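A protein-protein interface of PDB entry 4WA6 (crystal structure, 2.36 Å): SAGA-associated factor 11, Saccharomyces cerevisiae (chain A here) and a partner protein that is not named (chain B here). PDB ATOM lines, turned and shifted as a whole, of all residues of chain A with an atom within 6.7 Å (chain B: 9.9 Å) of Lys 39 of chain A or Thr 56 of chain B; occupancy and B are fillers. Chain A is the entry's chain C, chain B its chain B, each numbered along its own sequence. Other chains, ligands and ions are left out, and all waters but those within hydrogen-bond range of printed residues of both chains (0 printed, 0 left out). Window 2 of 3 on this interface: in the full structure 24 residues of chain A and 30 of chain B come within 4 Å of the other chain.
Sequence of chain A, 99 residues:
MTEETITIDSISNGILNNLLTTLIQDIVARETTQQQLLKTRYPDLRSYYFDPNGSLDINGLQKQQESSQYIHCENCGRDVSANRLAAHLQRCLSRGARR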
ATOM      1  N   GLU A  31       5.223  -8.560  16.748  1.00  0.00           N
ATOM      2  CA  GLU A  31       6.546  -8.081  16.388  1.00  0.00           C
ATOM      3  C   GLU A  31       7.552  -8.173  17.527  1.00  0.00           C
ATOM      4  O   GLU A  31       8.667  -8.677  17.345  1.00  0.00           O
ATOM      5  CB  GLU A  31       6.492  -6.636  15.948  1.00  0.00           C
ATOM      6  CG  GLU A  31       5.769  -6.395  14.633  1.00  0.00           C
ATOM      7  CD  GLU A  31       6.518  -6.926  13.413  1.00  0.00           C
ATOM      8  OE1 GLU A  31       7.748  -6.626  13.264  1.00  0.00           O
ATOM      9  OE2 GLU A  31       5.849  -7.623  12.605  1.00  0.00           O
ATOM     10  N   THR A  32       7.172  -7.643  18.689  1.00  0.00           N
ATOM     11  CA  THR A  32       8.142  -7.453  19.758  1.00  0.00           C
ATOM     12  C   THR A  32       8.519  -8.775  20.338  1.00  0.00           C
ATOM     13  O   THR A  32       9.663  -8.963  20.628  1.00  0.00           O
ATOM     14  CB  THR A  32       7.663  -6.519  20.893  1.00  0.00           C
ATOM     15  OG1 THR A  32       6.391  -6.952  21.433  1.00  0.00           O
ATOM     16  CG2 THR A  32       7.560  -5.139  20.387  1.00  0.00           C
ATOM     17  N   THR A  33       7.564  -9.698  20.496  1.00  0.00           N
ATOM     18  CA  THR A  33       7.946 -11.012  21.014  1.00  0.00           C
ATOM     19  C   THR A  33       8.749 -11.794  19.991  1.00  0.00           C
ATOM     20  O   THR A  33       9.573 -12.597  20.361  1.00  0.00           O
ATOM     21  CB  THR A  33       6.781 -11.889  21.461  1.00  0.00           C
ATOM     22  OG1 THR A  33       5.877 -12.072  20.369  1.00  0.00           O
ATOM     23  CG2 THR A  33       6.072 -11.279  22.569  1.00  0.00           C
ATOM     24  N   GLN A  34       8.529 -11.547  18.714  1.00  0.00           N
ATOM     25  CA  GLN A  34       9.318 -12.236  17.710  1.00  0.00           C
ATOM     26  C   GLN A  34      10.756 -11.762  17.860  1.00  0.00           C
ATOM     27  O   GLN A  34      11.682 -12.571  17.875  1.00  0.00           O
ATOM     28  CB  GLN A  34       8.808 -11.981  16.286  1.00  0.00           C
ATOM     29  CG  GLN A  34       9.707 -12.556  15.182  1.00  0.00           C
ATOM     30  CD  GLN A  34       9.887 -14.095  15.251  1.00  0.00           C
ATOM     31  OE1 GLN A  34      11.011 -14.619  15.183  1.00  0.00           O
ATOM     32  NE2 GLN A  34       8.787 -14.819  15.385  1.00  0.00           N
ATOM     33  N   GLN A  35      10.927 -10.450  17.972  1.00  0.00           N
ATOM     34  CA  GLN A  35      12.252  -9.870  18.145  1.00  0.00           C
ATOM     35  C   GLN A  35      12.953 -10.270  19.424  1.00  0.00           C
ATOM     36  O   GLN A  35      14.191 -10.452  19.441  1.00  0.00           O
ATOM     37  CB  GLN A  35      12.185  -8.356  18.114  1.00  0.00           C
ATOM     38  CG  GLN A  35      12.497  -7.769  16.778  1.00  0.00           C
ATOM     39  CD  GLN A  35      13.855  -8.199  16.260  1.00  0.00           C
ATOM     40  OE1 GLN A  35      14.919  -7.856  16.820  1.00  0.00           O
ATOM     41  NE2 GLN A  35      13.823  -8.956  15.171  1.00  0.00           N
ATOM     42  N   GLN A  36      12.183 -10.339  20.506  1.00  0.00           N
ATOM     43  CA  GLN A  36      12.719 -10.694  21.811  1.00  0.00           C
ATOM     44  C   GLN A  36      13.233 -12.109  21.654  1.00  0.00           C
ATOM     45  O   GLN A  36      14.358 -12.404  22.017  1.00  0.00           O
ATOM     46  CB  GLN A  36      11.637 -10.663  22.867  1.00  0.00           C
ATOM     47  CG  GLN A  36      11.994 -11.237  24.233  1.00  0.00           C
ATOM     48  CD  GLN A  36      10.749 -11.523  25.083  1.00  0.00           C
ATOM     49  OE1 GLN A  36      10.556 -12.627  25.553  1.00  0.00           O
ATOM     50  NE2 GLN A  36       9.894 -10.521  25.265  1.00  0.00           N
ATOM     51  N   LEU A  37      12.419 -12.970  21.047  1.00  0.00           N
ATOM     52  CA  LEU A  37      12.864 -14.345  20.762  1.00  0.00           C
ATOM     53  C   LEU A  37      14.115 -14.449  19.900  1.00  0.00           C
ATOM     54  O   LEU A  37      15.023 -15.155  20.253  1.00  0.00           O
ATOM     55  CB  LEU A  37      11.758 -15.180  20.127  1.00  0.00           C
ATOM     56  CG  LEU A  37      12.123 -16.653  20.018  1.00  0.00           C
ATOM     57  CD1 LEU A  37      12.273 -17.273  21.405  1.00  0.00           C
ATOM     58  CD2 LEU A  37      11.096 -17.420  19.177  1.00  0.00           C
ATOM     59  N   LEU A  38      14.160 -13.777  18.775  1.00  0.00           N
ATOM     60  CA  LEU A  38      15.281 -13.890  17.893  1.00  0.00           C
ATOM     61  C   LEU A  38      16.566 -13.377  18.557  1.00  0.00           C
ATOM     62  O   LEU A  38      17.618 -13.983  18.402  1.00  0.00           O
ATOM     63  CB  LEU A  38      15.035 -13.130  16.598  1.00  0.00           C
ATOM     64  CG  LEU A  38      14.087 -13.736  15.595  1.00  0.00           C
ATOM     65  CD1 LEU A  38      14.032 -12.803  14.372  1.00  0.00           C
ATOM     66  CD2 LEU A  38      14.484 -15.145  15.181  1.00  0.00           C
ATOM     67  N   LYS A  39      16.490 -12.280  19.300  1.00  0.00           N
ATOM     68  CA  LYS A  39      17.671 -11.772  19.966  1.00  0.00           C
ATOM     69  C   LYS A  39      18.057 -12.618  21.180  1.00  0.00           C
ATOM     70  O   LYS A  39      19.245 -12.640  21.541  1.00  0.00           O
ATOM     71  CB  LYS A  39      17.543 -10.282  20.319  1.00  0.00           C
ATOM     72  CG  LYS A  39      17.467  -9.379  19.082  1.00  0.00           C
ATOM     73  CD  LYS A  39      17.910  -7.935  19.359  1.00  0.00           C
ATOM     74  CE  LYS A  39      16.795  -7.056  19.939  1.00  0.00           C
ATOM     75  NZ  LYS A  39      17.324  -5.917  20.774  1.00  0.00           N
ATOM     76  N   THR A  40      17.123 -13.333  21.804  1.00  0.00           N
ATOM     77  CA  THR A  40      17.519 -14.243  22.903  1.00  0.00           C
ATOM     78  C   THR A  40      18.161 -15.557  22.391  1.00  0.00           C
ATOM     79  O   THR A  40      19.280 -15.921  22.759  1.00  0.00           O
ATOM     80  CB  THR A  40      16.340 -14.592  23.787  1.00  0.00           C
ATOM     81  OG1 THR A  40      15.614 -13.402  24.076  1.00  0.00           O
ATOM     82  CG2 THR A  40      16.836 -15.201  25.078  1.00  0.00           C
ATOM     83  N   ARG A  41      17.431 -16.243  21.523  1.00  0.00           N
ATOM     84  CA  ARG A  41      17.886 -17.438  20.799  1.00  0.00           C
ATOM     85  C   ARG A  41      19.259 -17.304  20.165  1.00  0.00           C
ATOM     86  O   ARG A  41      20.067 -18.212  20.259  1.00  0.00           O
ATOM     87  CB  ARG A  41      16.867 -17.762  19.678  1.00  0.00           C
ATOM     88  CG  ARG A  41      17.302 -18.895  18.764  1.00  0.00           C
ATOM     89  CD  ARG A  41      16.148 -19.499  17.999  1.00  0.00           C
ATOM     90  NE  ARG A  41      15.111 -19.997  18.913  1.00  0.00           N
ATOM     91  CZ  ARG A  41      13.899 -20.403  18.545  1.00  0.00           C
ATOM     92  NH1 ARG A  41      13.562 -20.403  17.257  1.00  0.00           N
ATOM     93  NH2 ARG A  41      13.044 -20.858  19.449  1.00  0.00           N
ATOM     94  N   TYR A  42      19.471 -16.186  19.469  1.00  0.00           N
ATOM     95  CA  TYR A  42      20.735 -15.887  18.782  1.00  0.00           C
ATOM     96  C   TYR A  42      21.412 -14.611  19.327  1.00  0.00           C
ATOM     97  O   TYR A  42      21.297 -13.544  18.715  1.00  0.00           O
ATOM     98  CB  TYR A  42      20.521 -15.722  17.257  1.00  0.00           C
ATOM     99  CG  TYR A  42      19.701 -16.814  16.622  1.00  0.00           C
ATOM    100  CD1 TYR A  42      20.175 -18.099  16.516  1.00  0.00           C
ATOM    101  CD2 TYR A  42      18.446 -16.544  16.104  1.00  0.00           C
ATOM    102  CE1 TYR A  42      19.402 -19.106  15.937  1.00  0.00           C
ATOM    103  CE2 TYR A  42      17.687 -17.526  15.524  1.00  0.00           C
ATOM    104  CZ  TYR A  42      18.152 -18.815  15.459  1.00  0.00           C
ATOM    105  OH  TYR A  42      17.346 -19.782  14.858  1.00  0.00           O
ATOM    106  N   PRO A  43      22.147 -14.723  20.449  1.00  0.00           N
ATOM    107  CA  PRO A  43      22.949 -13.591  20.979  1.00  0.00           C
ATOM    108  C   PRO A  43      23.809 -12.919  19.886  1.00  0.00           C
ATOM    109  O   PRO A  43      23.935 -11.701  19.838  1.00  0.00           O
ATOM    110  CB  PRO A  43      23.868 -14.257  21.995  1.00  0.00           C
ATOM    111  CG  PRO A  43      23.167 -15.507  22.402  1.00  0.00           C
ATOM    112  CD  PRO A  43      22.382 -15.970  21.205  1.00  0.00           C
ATOM    113  N   ASP A  44      24.327 -13.744  18.991  1.00  0.00           N
ATOM    114  CA  ASP A  44      25.242 -13.363  17.909  1.00  0.00           C
ATOM    115  C   ASP A  44      24.599 -12.787  16.621  1.00  0.00           C
ATOM    116  O   ASP A  44      25.277 -12.688  15.588  1.00  0.00           O
ATOM    117  CB  ASP A  44      25.961 -14.661  17.517  1.00  0.00           C
ATOM    118  CG  ASP A  44      24.963 -15.838  17.316  1.00  0.00           C
ATOM    119  OD1 ASP A  44      24.034 -15.985  18.155  1.00  0.00           O
ATOM    120  OD2 ASP A  44      25.096 -16.605  16.329  1.00  0.00           O
ATOM    121  N   LEU A  45      23.320 -12.413  16.672  1.00  0.00           N
ATOM    122  CA  LEU A  45      22.509 -12.243  15.473  1.00  0.00           C
ATOM    123  C   LEU A  45      22.972 -11.154  14.495  1.00  0.00           C
ATOM    124  O   LEU A  45      23.182 -10.009  14.892  1.00  0.00           O
ATOM    125  CB  LEU A  45      21.067 -11.935  15.883  1.00  0.00           C
ATOM    126  CG  LEU A  45      20.039 -11.817  14.753  1.00  0.00           C
ATOM    127  CD1 LEU A  45      19.968 -13.112  13.960  1.00  0.00           C
ATOM    128  CD2 LEU A  45      18.671 -11.477  15.307  1.00  0.00           C
ATOM    129  N   THR B  46       6.541  -0.325  13.738  1.00  0.00           N
ATOM    130  CA  THR B  46       7.021  -1.055  14.908  1.00  0.00           C
ATOM    131  C   THR B  46       8.513  -1.420  14.810  1.00  0.00           C
ATOM    132  O   THR B  46       9.297  -1.249  15.779  1.00  0.00           O
ATOM    133  CB  THR B  46       6.202  -2.312  15.132  1.00  0.00           C
ATOM    134  OG1 THR B  46       4.812  -1.976  15.151  1.00  0.00           O
ATOM    135  CG2 THR B  46       6.518  -2.938  16.424  1.00  0.00           C
ATOM    136  N   LYS B  47       8.912  -1.939  13.652  1.00  0.00           N
ATOM    137  CA  LYS B  47      10.303  -2.351  13.497  1.00  0.00           C
ATOM    138  C   LYS B  47      11.212  -1.120  13.611  1.00  0.00           C
ATOM    139  O   LYS B  47      12.291  -1.177  14.184  1.00  0.00           O
ATOM    140  CB  LYS B  47      10.542  -3.065  12.161  1.00  0.00           C
ATOM    141  CG  LYS B  47      10.125  -4.531  12.157  1.00  0.00           C
ATOM    142  CD  LYS B  47      10.276  -5.194  10.778  1.00  0.00           C
ATOM    143  CE  LYS B  47       9.717  -6.616  10.731  1.00  0.00           C
ATOM    144  NZ  LYS B  47       8.263  -6.610  10.448  1.00  0.00           N
ATOM    145  N   GLU B  49      10.626   1.555  15.277  1.00  0.00           N
ATOM    146  CA  GLU B  49      10.633   2.000  16.663  1.00  0.00           C
ATOM    147  C   GLU B  49      11.413   1.087  17.577  1.00  0.00           C
ATOM    148  O   GLU B  49      12.051   1.595  18.497  1.00  0.00           O
ATOM    149  CB  GLU B  49       9.224   2.239  17.225  1.00  0.00           C
ATOM    150  CG  GLU B  49       8.456   3.375  16.558  1.00  0.00           C
ATOM    151  CD  GLU B  49       8.912   4.779  16.949  1.00  0.00           C
ATOM    152  OE1 GLU B  49       9.450   5.016  18.068  1.00  0.00           O
ATOM    153  OE2 GLU B  49       8.709   5.672  16.105  1.00  0.00           O
ATOM    154  N   MET B  50      11.400  -0.223  17.352  1.00  0.00           N
ATOM    155  CA  MET B  50      12.352  -1.096  18.061  1.00  0.00           C
ATOM    156  C   MET B  50      13.809  -0.722  17.777  1.00  0.00           C
ATOM    157  O   MET B  50      14.632  -0.715  18.700  1.00  0.00           O
ATOM    158  CB  MET B  50      12.162  -2.584  17.771  1.00  0.00           C
ATOM    159  CG  MET B  50      10.848  -3.157  18.300  1.00  0.00           C
ATOM    160  SD  MET B  50      10.764  -4.953  18.117  1.00  0.00           S
ATOM    161  CE  MET B  50      10.687  -5.043  16.315  1.00  0.00           C
ATOM    162  N   ASN B  51      14.125  -0.422  16.524  1.00  0.00           N
ATOM    163  CA  ASN B  51      15.513  -0.214  16.127  1.00  0.00           C
ATOM    164  C   ASN B  51      16.057   1.068  16.746  1.00  0.00           C
ATOM    165  O   ASN B  51      17.113   1.054  17.409  1.00  0.00           O
ATOM    166  CB  ASN B  51      15.665  -0.176  14.604  1.00  0.00           C
ATOM    167  CG  ASN B  51      15.585  -1.557  13.978  1.00  0.00           C
ATOM    168  OD1 ASN B  51      15.881  -2.579  14.621  1.00  0.00           O
ATOM    169  ND2 ASN B  51      15.186  -1.604  12.710  1.00  0.00           N
ATOM    170  N   ILE B  52      15.287   2.141  16.553  1.00  0.00           N
ATOM    171  CA  ILE B  52      15.571   3.471  17.100  1.00  0.00           C
ATOM    172  C   ILE B  52      15.728   3.424  18.611  1.00  0.00           C
ATOM    173  O   ILE B  52      16.707   3.946  19.161  1.00  0.00           O
ATOM    174  CB  ILE B  52      14.449   4.462  16.723  1.00  0.00           C
ATOM    175  CG1 ILE B  52      14.562   4.841  15.250  1.00  0.00           C
ATOM    176  CG2 ILE B  52      14.512   5.730  17.560  1.00  0.00           C
ATOM    177  CD1 ILE B  52      13.283   5.395  14.644  1.00  0.00           C
ATOM    178  N   ASN B  53      14.778   2.790  19.296  1.00  0.00           N
ATOM    179  CA  ASN B  53      14.842   2.739  20.764  1.00  0.00           C
ATOM    180  C   ASN B  53      15.692   1.575  21.291  1.00  0.00           C
ATOM    181  O   ASN B  53      15.818   1.420  22.506  1.00  0.00           O
ATOM    182  CB  ASN B  53      13.444   2.708  21.365  1.00  0.00           C
ATOM    183  CG  ASN B  53      12.705   4.008  21.151  1.00  0.00           C
ATOM    184  OD1 ASN B  53      12.954   4.975  21.871  1.00  0.00           O
ATOM    185  ND2 ASN B  53      11.787   4.047  20.183  1.00  0.00           N
ATOM    186  N   GLU B  54      16.305   0.800  20.390  1.00  0.00           N
ATOM    187  CA  GLU B  54      17.095  -0.368  20.785  1.00  0.00           C
ATOM    188  C   GLU B  54      16.378  -1.023  21.946  1.00  0.00           C
ATOM    189  O   GLU B  54      16.960  -1.191  23.021  1.00  0.00           O
ATOM    190  CB  GLU B  54      18.538   0.000  21.169  1.00  0.00           C
ATOM    191  CG  GLU B  54      19.444   0.262  19.979  1.00  0.00           C
ATOM    192  CD  GLU B  54      20.852   0.822  20.334  1.00  0.00           C
ATOM    193  OE1 GLU B  54      21.090   1.340  21.469  1.00  0.00           O
ATOM    194  OE2 GLU B  54      21.745   0.745  19.441  1.00  0.00           O
ATOM    195  N   SER B  55      15.102  -1.368  21.724  1.00  0.00           N
ATOM    196  CA  SER B  55      14.309  -2.046  22.740  1.00  0.00           C
ATOM    197  C   SER B  55      13.243  -2.959  22.134  1.00  0.00           C
ATOM    198  O   SER B  55      12.719  -2.653  21.076  1.00  0.00           O
ATOM    199  CB  SER B  55      13.658  -1.026  23.661  1.00  0.00           C
ATOM    200  OG  SER B  55      12.808  -1.667  24.599  1.00  0.00           O
ATOM    201  N   THR B  56      12.969  -4.077  22.805  1.00  0.00           N
ATOM    202  CA  THR B  56      11.887  -4.947  22.444  1.00  0.00           C
ATOM    203  C   THR B  56      10.805  -4.955  23.504  1.00  0.00           C
ATOM    204  O   THR B  56       9.876  -5.758  23.427  1.00  0.00           O
ATOM    205  CB  THR B  56      12.349  -6.403  22.202  1.00  0.00           C
ATOM    206  OG1 THR B  56      12.721  -7.009  23.444  1.00  0.00           O
ATOM    207  CG2 THR B  56      13.496  -6.425  21.247  1.00  0.00           C
ATOM    208  N   ASN B  57      10.900  -4.057  24.474  1.00  0.00           N
ATOM    209  CA  ASN B  57       9.913  -4.015  25.546  1.00  0.00           C
ATOM    210  C   ASN B  57       8.583  -3.535  25.010  1.00  0.00           C
ATOM    211  O   ASN B  57       8.464  -2.419  24.497  1.00  0.00           O
ATOM    212  CB  ASN B  57      10.374  -3.120  26.713  1.00  0.00           C
ATOM    213  CG  ASN B  57       9.273  -2.942  27.768  1.00  0.00           C
ATOM    214  OD1 ASN B  57       8.332  -2.173  27.585  1.00  0.00           O
ATOM    215  ND2 ASN B  57       9.340  -3.722  28.824  1.00  0.00           N
ATOM    216  N   PHE B  58       7.584  -4.415  25.120  1.00  0.00           N
ATOM    217  CA  PHE B  58       6.308  -4.194  24.519  1.00  0.00           C
ATOM    218  C   PHE B  58       5.778  -2.808  24.914  1.00  0.00           C
ATOM    219  O   PHE B  58       5.330  -2.029  24.088  1.00  0.00           O
ATOM    220  CB  PHE B  58       5.305  -5.299  24.927  1.00  0.00           C
ATOM    221  CG  PHE B  58       3.928  -5.007  24.471  1.00  0.00           C
ATOM    222  CD1 PHE B  58       3.588  -5.186  23.134  1.00  0.00           C
ATOM    223  CD2 PHE B  58       3.022  -4.406  25.325  1.00  0.00           C
ATOM    224  CE1 PHE B  58       2.358  -4.818  22.684  1.00  0.00           C
ATOM    225  CE2 PHE B  58       1.758  -4.053  24.880  1.00  0.00           C
ATOM    226  CZ  PHE B  58       1.426  -4.248  23.558  1.00  0.00           C
ATOM    227  N   THR B  59       5.862  -2.481  26.179  1.00  0.00           N
ATOM    228  CA  THR B  59       5.112  -1.307  26.735  1.00  0.00           C
ATOM    229  C   THR B  59       5.745  -0.034  26.220  1.00  0.00           C
ATOM    230  O   THR B  59       5.101   0.843  25.675  1.00  0.00           O
ATOM    231  CB  THR B  59       5.130  -1.380  28.258  1.00  0.00           C
ATOM    232  OG1 THR B  59       4.419  -2.565  28.682  1.00  0.00           O
ATOM    233  CG2 THR B  59       4.553  -0.142  28.896  1.00  0.00           C
ATOM    234  N   GLN B  60       7.054   0.010  26.324  1.00  0.00           N
ATOM    235  CA  GLN B  60       7.799   1.079  25.762  1.00  0.00           C
ATOM    236  C   GLN B  60       7.501   1.262  24.255  1.00  0.00           C
ATOM    237  O   GLN B  60       7.223   2.379  23.787  1.00  0.00           O
ATOM    238  CB  GLN B  60       9.265   0.827  26.026  1.00  0.00           C
ATOM    239  CG  GLN B  60      10.140   1.865  25.394  1.00  0.00           C
ATOM    240  CD  GLN B  60      11.607   1.602  25.643  1.00  0.00           C
ATOM    241  OE1 GLN B  60      11.979   0.583  26.250  1.00  0.00           O
ATOM    242  NE2 GLN B  60      12.460   2.524  25.184  1.00  0.00           N
ATOM    243  N   ILE B  61       7.520   0.177  23.501  1.00  0.00           N
ATOM    244  CA  ILE B  61       7.398   0.282  22.058  1.00  0.00           C
ATOM    245  C   ILE B  61       6.002   0.719  21.622  1.00  0.00           C
ATOM    246  O   ILE B  61       5.834   1.586  20.752  1.00  0.00           O
ATOM    247  CB  ILE B  61       7.798  -1.046  21.424  1.00  0.00           C
ATOM    248  CG1 ILE B  61       9.296  -1.275  21.653  1.00  0.00           C
ATOM    249  CG2 ILE B  61       7.467  -1.095  19.945  1.00  0.00           C
ATOM    250  CD1 ILE B  61      10.224  -0.220  21.050  1.00  0.00           C
ATOM    251  N   LEU B  62       5.006   0.172  22.287  1.00  0.00           N
ATOM    252  CA  LEU B  62       3.640   0.522  21.994  1.00  0.00           C
ATOM    253  C   LEU B  62       3.441   1.973  22.253  1.00  0.00           C
ATOM    254  O   LEU B  62       2.696   2.661  21.550  1.00  0.00           O
ATOM    255  CB  LEU B  62       2.705  -0.249  22.944  1.00  0.00           C
ATOM    256  CG  LEU B  62       1.230  -0.046  22.785  1.00  0.00           C
ATOM    257  CD1 LEU B  62       0.880  -0.756  21.479  1.00  0.00           C
ATOM    258  CD2 LEU B  62       0.411  -0.558  23.979  1.00  0.00           C
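The side-chain carboxylate of Glu 31 of chain A is in salt-bridge range of the side-chain amino group of Lys 47 of chain B, at 2.9 Å.
O of Gln 36 of chain A sits at hydrogen-bond distance from OG1 of Thr 40 of chain A. The backbone carbonyl oxygen (O) of Met 50 of chain B is in hydrogen-bond range of the backbone NH (N) of Ser 55 of chain B (3.1 Å). The backbone carbonyl oxygen (O) of Lys 47 of chain B lies within hydrogen-bond range of the side-chain amide nitrogen (ND2) of Asn 51 of chain B (3.3 Å).
Thr 46 of chain B touches Glu 31 of chain A. Thr 32 of chain A touches Met 50 of chain B. O of Thr 56 of chain B touches CB of Thr 32 of chain A (3.4 Å). CD1 of Phe 58 of chain B touches OG1 of Thr 32 of chain A (3.7 Å). Met 50 of chain B touches Gln 35 of chain A. CB of Gln 35 of chain A touches CG2 of Thr 56 of chain B (3.9 Å). CB of Gln 36 of chain A touches OG1 of Thr 56 of chain B, 3.9 Å away. CG2 of Thr 56 of chain B touches CE of Lys 39 of chain A, 3.6 Å away.
Of chain B, only Thr 56 (3.6 Å) comes within 4 Å of Lys 39 of chain A. Of chain A, only Thr 32, Gln 35, Gln 36 and Lys 39 come within 4 Å of Thr 56 of chain B. Thr 32 of chain A touches just these residues of chain B: Met 50 (3.9 Å), Thr 56 (3.4 Å) and Phe 58 (3.7 Å). Of chain B, only Met 50 (3.3 Å) and Thr 56 (3.9 Å) come within 4 Å of Gln 35 of chain A. Leu 38 of chain A touches none of the printed residues of chain B. No residue of chain B comes within 4 Å of Thr 40 of chain A. No residue of chain B comes within 4 Å of Pro 43 of chain A. Of the printed residues of chain A, Lys 47 of chain B touches Glu 31. Of the printed residues of chain A, Met 50 of chain B touches Thr 32 (3.9 Å) and Gln 35 (3.3 Å). Of the printed residues of chain A, Thr 46 of chain B touches Glu 31. Of the printed residues of chain B, Gln 36 of chain A touches Thr 56 (3.9 Å). Of the printed residues of chain A, Phe 58 of chain B touches Thr 32. Asn 51 of chain B touches none of the printed residues of chain A. The nearest printed residue of chain B that does not touch Gln 36 of chain A is Met 50 of chain B (6.1 Å).
Of the 16 printed residues of chain B, 5 touch a printed residue of chain A. Printed residues of chain A that touch a printed residue of chain B: Glu 31, Thr 32, Gln 35, Gln 36 and Lys 39. Among the printed residues, Asp or Glu carboxylates within 4 Å of a Lys or Arg side-chain nitrogen of the other chain: Glu 31 of chain A with Lys 47 of chain B.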
